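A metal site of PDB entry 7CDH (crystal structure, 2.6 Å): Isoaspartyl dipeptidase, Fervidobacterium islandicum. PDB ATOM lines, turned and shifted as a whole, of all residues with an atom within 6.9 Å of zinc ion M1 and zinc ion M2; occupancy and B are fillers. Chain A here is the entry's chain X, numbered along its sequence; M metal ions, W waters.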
ATOM      1  N   HIS A  61      24.389  19.069  24.523  1.00  0.00           N
ATOM      2  CA  HIS A  61      24.931  19.102  23.152  1.00  0.00           C
ATOM      3  C   HIS A  61      23.877  19.587  22.137  1.00  0.00           C
ATOM      4  O   HIS A  61      23.138  18.749  21.599  1.00  0.00           O
ATOM      5  CB  HIS A  61      25.491  17.726  22.822  1.00  0.00           C
ATOM      6  CG  HIS A  61      26.158  17.688  21.504  1.00  0.00           C
ATOM      7  ND1 HIS A  61      27.513  17.825  21.374  1.00  0.00           N
ATOM      8  CD2 HIS A  61      25.659  17.596  20.259  1.00  0.00           C
ATOM      9  CE1 HIS A  61      27.825  17.771  20.108  1.00  0.00           C
ATOM     10  NE2 HIS A  61      26.707  17.669  19.394  1.00  0.00           N
ATOM     11  N   VAL A  62      23.826  20.917  21.905  1.00  0.00           N
ATOM     12  CA  VAL A  62      22.896  21.586  20.940  1.00  0.00           C
ATOM     13  C   VAL A  62      23.648  22.559  20.029  1.00  0.00           C
ATOM     14  O   VAL A  62      24.425  23.368  20.501  1.00  0.00           O
ATOM     15  CB  VAL A  62      21.770  22.315  21.679  1.00  0.00           C
ATOM     16  CG1 VAL A  62      20.786  22.943  20.726  1.00  0.00           C
ATOM     17  CG2 VAL A  62      21.056  21.352  22.612  1.00  0.00           C
ATOM     18  N   HIS A  63      23.417  22.464  18.728  1.00  0.00           N
ATOM     19  CA  HIS A  63      23.959  23.428  17.746  1.00  0.00           C
ATOM     20  C   HIS A  63      23.039  24.627  17.751  1.00  0.00           C
ATOM     21  O   HIS A  63      22.314  24.736  16.817  1.00  0.00           O
ATOM     22  CB  HIS A  63      24.131  22.773  16.386  1.00  0.00           C
ATOM     23  CG  HIS A  63      25.150  21.683  16.448  1.00  0.00           C
ATOM     24  ND1 HIS A  63      26.479  21.953  16.566  1.00  0.00           N
ATOM     25  CD2 HIS A  63      25.036  20.340  16.471  1.00  0.00           C
ATOM     26  CE1 HIS A  63      27.171  20.816  16.614  1.00  0.00           C
ATOM     27  NE2 HIS A  63      26.307  19.806  16.557  1.00  0.00           N
ATOM     28  N   CYS A  96      27.501  24.222  20.993  1.00  0.00           N
ATOM     29  CA  CYS A  96      28.810  24.081  20.332  1.00  0.00           C
ATOM     30  C   CYS A  96      28.675  24.303  18.827  1.00  0.00           C
ATOM     31  O   CYS A  96      27.525  24.369  18.316  1.00  0.00           O
ATOM     32  CB  CYS A  96      29.361  22.693  20.616  1.00  0.00           C
ATOM     33  SG  CYS A  96      28.263  21.370  20.052  1.00  0.00           S
ATOM     34  N   LEU A  97      29.826  24.334  18.152  1.00  0.00           N
ATOM     35  CA  LEU A  97      29.948  24.242  16.678  1.00  0.00           C
ATOM     36  C   LEU A  97      30.278  22.810  16.251  1.00  0.00           C
ATOM     37  O   LEU A  97      30.797  22.033  17.062  1.00  0.00           O
ATOM     38  CB  LEU A  97      31.062  25.175  16.172  1.00  0.00           C
ATOM     39  CG  LEU A  97      30.965  26.615  16.632  1.00  0.00           C
ATOM     40  CD1 LEU A  97      32.117  27.417  16.069  1.00  0.00           C
ATOM     41  CD2 LEU A  97      29.636  27.195  16.187  1.00  0.00           C
ATOM     42  N   GLY A  98      30.057  22.515  14.978  1.00  0.00           N
ATOM     43  CA  GLY A  98      30.219  21.170  14.424  1.00  0.00           C
ATOM     44  C   GLY A  98      31.183  21.156  13.260  1.00  0.00           C
ATOM     45  O   GLY A  98      32.220  21.763  13.342  1.00  0.00           O
ATOM     46  N   TYR A 130      34.757  20.903  15.315  1.00  0.00           N
ATOM     47  CA  TYR A 130      35.270  19.572  14.908  1.00  0.00           C
ATOM     48  C   TYR A 130      36.776  19.632  14.723  1.00  0.00           C
ATOM     49  O   TYR A 130      37.467  18.728  15.152  1.00  0.00           O
ATOM     50  CB  TYR A 130      34.678  19.104  13.571  1.00  0.00           C
ATOM     51  CG  TYR A 130      33.427  18.272  13.618  1.00  0.00           C
ATOM     52  CD1 TYR A 130      32.442  18.426  14.587  1.00  0.00           C
ATOM     53  CD2 TYR A 130      33.206  17.328  12.625  1.00  0.00           C
ATOM     54  CE1 TYR A 130      31.278  17.678  14.581  1.00  0.00           C
ATOM     55  CE2 TYR A 130      32.061  16.543  12.613  1.00  0.00           C
ATOM     56  CZ  TYR A 130      31.091  16.721  13.581  1.00  0.00           C
ATOM     57  OH  TYR A 130      29.955  15.950  13.498  1.00  0.00           O
ATOM     58  N   GLU A 156      32.808  20.426  19.486  1.00  0.00           N
ATOM     59  CA  GLU A 156      32.995  18.992  19.634  1.00  0.00           C
ATOM     60  C   GLU A 156      34.138  18.556  18.709  1.00  0.00           C
ATOM     61  O   GLU A 156      33.996  18.662  17.495  1.00  0.00           O
ATOM     62  CB  GLU A 156      31.690  18.217  19.432  1.00  0.00           C
ATOM     63  CG  GLU A 156      30.884  18.664  18.252  1.00  0.00           C
ATOM     64  CD  GLU A 156      29.735  17.771  17.788  1.00  0.00           C
ATOM     65  OE1 GLU A 156      29.763  16.506  18.003  1.00  0.00           O
ATOM     66  OE2 GLU A 156      28.785  18.366  17.251  1.00  0.00           O
ATOM     67  N   ARG A 163      34.957  13.354   8.721  1.00  0.00           N
ATOM     68  CA  ARG A 163      34.946  14.843   8.768  1.00  0.00           C
ATOM     69  C   ARG A 163      35.983  15.388   9.770  1.00  0.00           C
ATOM     70  O   ARG A 163      36.064  16.654   9.963  1.00  0.00           O
ATOM     71  CB  ARG A 163      33.550  15.364   9.109  1.00  0.00           C
ATOM     72  CG  ARG A 163      32.484  15.015   8.077  1.00  0.00           C
ATOM     73  CD  ARG A 163      31.116  15.042   8.745  1.00  0.00           C
ATOM     74  NE  ARG A 163      30.936  13.838   9.567  1.00  0.00           N
ATOM     75  CZ  ARG A 163      29.847  13.546  10.279  1.00  0.00           C
ATOM     76  NH1 ARG A 163      28.818  14.369  10.331  1.00  0.00           N
ATOM     77  NH2 ARG A 163      29.812  12.407  10.952  1.00  0.00           N
ATOM     78  N   ASN A 193      34.632  17.598  24.733  1.00  0.00           N
ATOM     79  CA  ASN A 193      33.545  16.834  24.099  1.00  0.00           C
ATOM     80  C   ASN A 193      34.103  16.281  22.781  1.00  0.00           C
ATOM     81  O   ASN A 193      34.541  17.084  21.928  1.00  0.00           O
ATOM     82  CB  ASN A 193      32.298  17.707  23.964  1.00  0.00           C
ATOM     83  CG  ASN A 193      31.134  17.024  23.279  1.00  0.00           C
ATOM     84  OD1 ASN A 193      30.479  17.627  22.435  1.00  0.00           O
ATOM     85  ND2 ASN A 193      30.806  15.819  23.680  1.00  0.00           N
ATOM     86  N   PHE A 194      34.135  14.953  22.660  1.00  0.00           N
ATOM     87  CA  PHE A 194      34.616  14.262  21.440  1.00  0.00           C
ATOM     88  C   PHE A 194      33.391  13.852  20.637  1.00  0.00           C
ATOM     89  O   PHE A 194      32.549  13.132  21.179  1.00  0.00           O
ATOM     90  CB  PHE A 194      35.439  13.028  21.786  1.00  0.00           C
ATOM     91  CG  PHE A 194      36.727  13.356  22.469  1.00  0.00           C
ATOM     92  CD1 PHE A 194      37.809  13.830  21.751  1.00  0.00           C
ATOM     93  CD2 PHE A 194      36.851  13.262  23.842  1.00  0.00           C
ATOM     94  CE1 PHE A 194      38.995  14.164  22.388  1.00  0.00           C
ATOM     95  CE2 PHE A 194      38.034  13.605  24.478  1.00  0.00           C
ATOM     96  CZ  PHE A 194      39.104  14.044  23.742  1.00  0.00           C
ATOM     97  N   HIS A 195      33.289  14.364  19.399  1.00  0.00           N
ATOM     98  CA  HIS A 195      32.443  13.732  18.375  1.00  0.00           C
ATOM     99  C   HIS A 195      33.115  12.422  17.965  1.00  0.00           C
ATOM    100  O   HIS A 195      34.219  12.465  17.397  1.00  0.00           O
ATOM    101  CB  HIS A 195      32.227  14.646  17.185  1.00  0.00           C
ATOM    102  CG  HIS A 195      31.647  13.939  16.011  1.00  0.00           C
ATOM    103  ND1 HIS A 195      30.300  13.979  15.744  1.00  0.00           N
ATOM    104  CD2 HIS A 195      32.223  13.133  15.088  1.00  0.00           C
ATOM    105  CE1 HIS A 195      30.071  13.241  14.671  1.00  0.00           C
ATOM    106  NE2 HIS A 195      31.238  12.705  14.229  1.00  0.00           N
ATOM    107  N   VAL A 196      32.478  11.296  18.232  1.00  0.00           N
ATOM    108  CA  VAL A 196      33.057   9.988  17.827  1.00  0.00           C
ATOM    109  C   VAL A 196      32.306   9.478  16.606  1.00  0.00           C
ATOM    110  O   VAL A 196      31.095   9.244  16.702  1.00  0.00           O
ATOM    111  CB  VAL A 196      33.047   8.950  18.945  1.00  0.00           C
ATOM    112  CG1 VAL A 196      33.771   7.695  18.472  1.00  0.00           C
ATOM    113  CG2 VAL A 196      33.667   9.490  20.227  1.00  0.00           C
ATOM    114  N   THR A 223      30.620  11.659  22.735  1.00  0.00           N
ATOM    115  CA  THR A 223      29.181  11.568  22.374  1.00  0.00           C
ATOM    116  C   THR A 223      29.033  10.599  21.186  1.00  0.00           C
ATOM    117  O   THR A 223      30.055  10.083  20.724  1.00  0.00           O
ATOM    118  CB  THR A 223      28.565  12.962  22.176  1.00  0.00           C
ATOM    119  OG1 THR A 223      27.157  12.790  21.965  1.00  0.00           O
ATOM    120  CG2 THR A 223      29.174  13.727  21.014  1.00  0.00           C
ATOM    121  N   HIS A 224      27.790  10.365  20.738  1.00  0.00           N
ATOM    122  CA  HIS A 224      27.427   9.377  19.690  1.00  0.00           C
ATOM    123  C   HIS A 224      27.852   7.980  20.129  1.00  0.00           C
ATOM    124  O   HIS A 224      28.170   7.171  19.294  1.00  0.00           O
ATOM    125  CB  HIS A 224      28.046   9.734  18.324  1.00  0.00           C
ATOM    126  CG  HIS A 224      27.785  11.157  18.012  1.00  0.00           C
ATOM    127  ND1 HIS A 224      26.527  11.701  18.097  1.00  0.00           N
ATOM    128  CD2 HIS A 224      28.630  12.169  17.716  1.00  0.00           C
ATOM    129  CE1 HIS A 224      26.588  12.983  17.875  1.00  0.00           C
ATOM    130  NE2 HIS A 224      27.861  13.297  17.624  1.00  0.00           N
ATOM    131  N   ARG A 227      26.122   4.855  18.717  1.00  0.00           N
ATOM    132  CA  ARG A 227      26.176   4.748  17.231  1.00  0.00           C
ATOM    133  C   ARG A 227      26.188   3.265  16.831  1.00  0.00           C
ATOM    134  O   ARG A 227      25.592   2.911  15.826  1.00  0.00           O
ATOM    135  CB  ARG A 227      27.382   5.570  16.770  1.00  0.00           C
ATOM    136  CG  ARG A 227      27.810   5.379  15.332  1.00  0.00           C
ATOM    137  CD  ARG A 227      29.173   6.004  15.038  1.00  0.00           C
ATOM    138  NE  ARG A 227      29.219   7.425  15.316  1.00  0.00           N
ATOM    139  CZ  ARG A 227      28.635   8.360  14.568  1.00  0.00           C
ATOM    140  NH1 ARG A 227      28.718   9.640  14.900  1.00  0.00           N
ATOM    141  NH2 ARG A 227      27.938   8.009  13.496  1.00  0.00           N
ATOM    142  N   THR A 248      23.249   9.882  21.683  1.00  0.00           N
ATOM    143  CA  THR A 248      22.360  10.808  20.949  1.00  0.00           C
ATOM    144  C   THR A 248      20.932  10.308  21.178  1.00  0.00           C
ATOM    145  O   THR A 248      20.630   9.154  20.813  1.00  0.00           O
ATOM    146  CB  THR A 248      22.763  10.937  19.481  1.00  0.00           C
ATOM    147  OG1 THR A 248      24.139  11.304  19.452  1.00  0.00           O
ATOM    148  CG2 THR A 248      21.913  11.967  18.780  1.00  0.00           C
ATOM    149  N   ASP A 285      21.491  16.685  20.066  1.00  0.00           N
ATOM    150  CA  ASP A 285      22.262  17.163  18.888  1.00  0.00           C
ATOM    151  C   ASP A 285      21.344  18.096  18.082  1.00  0.00           C
ATOM    152  O   ASP A 285      21.263  17.957  16.853  1.00  0.00           O
ATOM    153  CB  ASP A 285      22.749  15.979  18.065  1.00  0.00           C
ATOM    154  CG  ASP A 285      24.004  16.319  17.288  1.00  0.00           C
ATOM    155  OD1 ASP A 285      24.519  17.400  17.530  1.00  0.00           O
ATOM    156  OD2 ASP A 285      24.493  15.467  16.495  1.00  0.00           O
ATOM    157  N   GLY A 286      20.595  18.938  18.781  1.00  0.00           N
ATOM    158  CA  GLY A 286      19.523  19.737  18.169  1.00  0.00           C
ATOM    159  C   GLY A 286      20.094  20.669  17.111  1.00  0.00           C
ATOM    160  O   GLY A 286      21.173  21.189  17.374  1.00  0.00           O
ATOM    161  N   GLY A 288      21.395  19.802  14.544  1.00  0.00           N
ATOM    162  CA  GLY A 288      22.411  18.997  13.866  1.00  0.00           C
ATOM    163  C   GLY A 288      21.888  18.491  12.536  1.00  0.00           C
ATOM    164  O   GLY A 288      20.655  18.618  12.297  1.00  0.00           O
HETATM  165 ZN    ZN M   1      28.733  15.158  16.540  1.00  0.00          ZN
HETATM  166 ZN    ZN M   2      26.864  17.665  17.291  1.00  0.00          ZN
HETATM  167  O   HOH W   1      27.814  16.844  14.550  1.00  0.00           O
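The backbone NH (N) of Tyr 130 sits close to the backbone carbonyl oxygen (O) of Glu 156, 3.2 Å away.
OD1 of Asn 193 sits at hydrogen-bond distance from ND1 of His 61, 3.2 Å away.
A ring nitrogen (ND1) of His 195 lies close to the side-chain hydroxyl of Tyr 130, at 3.0 Å.
A ring nitrogen (ND1) of His 224 lies within hydrogen-bond range of the side-chain hydroxyl (OG1) of Thr 248 (2.8 Å).
ND1 of His 63 lies within hydrogen-bond range of O of Cys 96 (3.2 Å).
The backbone carbonyl oxygen (O) of Gly 286 is in hydrogen-bond range of the backbone NH (N) of His 63, 2.9 Å away.
The backbone NH (N) of Tyr 130 sits at hydrogen-bond distance from the backbone carbonyl oxygen (O) of Gly 98 (3.3 Å).
Residues that only touch zinc ion M1: Tyr 130 (3.4 Å).
Four residues have an atom within 4 Å of zinc ion M1: Tyr 130, Glu 156, His 195 and His 224.
The nearest printed residue that does not touch zinc ion M1 is Asp 285 (4.3 Å).
Of the 20 residues printed, 4 come within 4 Å of zinc ion M2.
The nearest printed residue that does not touch zinc ion M2 is His 224 (4.5 Å).
Zinc ion M1 is bound by a ring nitrogen (ND1) of His 195, the side-chain carboxylate (OE1) of Glu 156 and a ring nitrogen (NE2) of His 224.
Slightly farther from zinc ion M1 lies water W1 (2.8 Å).
Zinc ion M2 is bound by OE2 of Glu 156 (2.0 Å), NE2 of His 61 (2.1 Å), NE2 of His 63 (2.3 Å) and OD1 of Asp 285 (2.4 Å).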
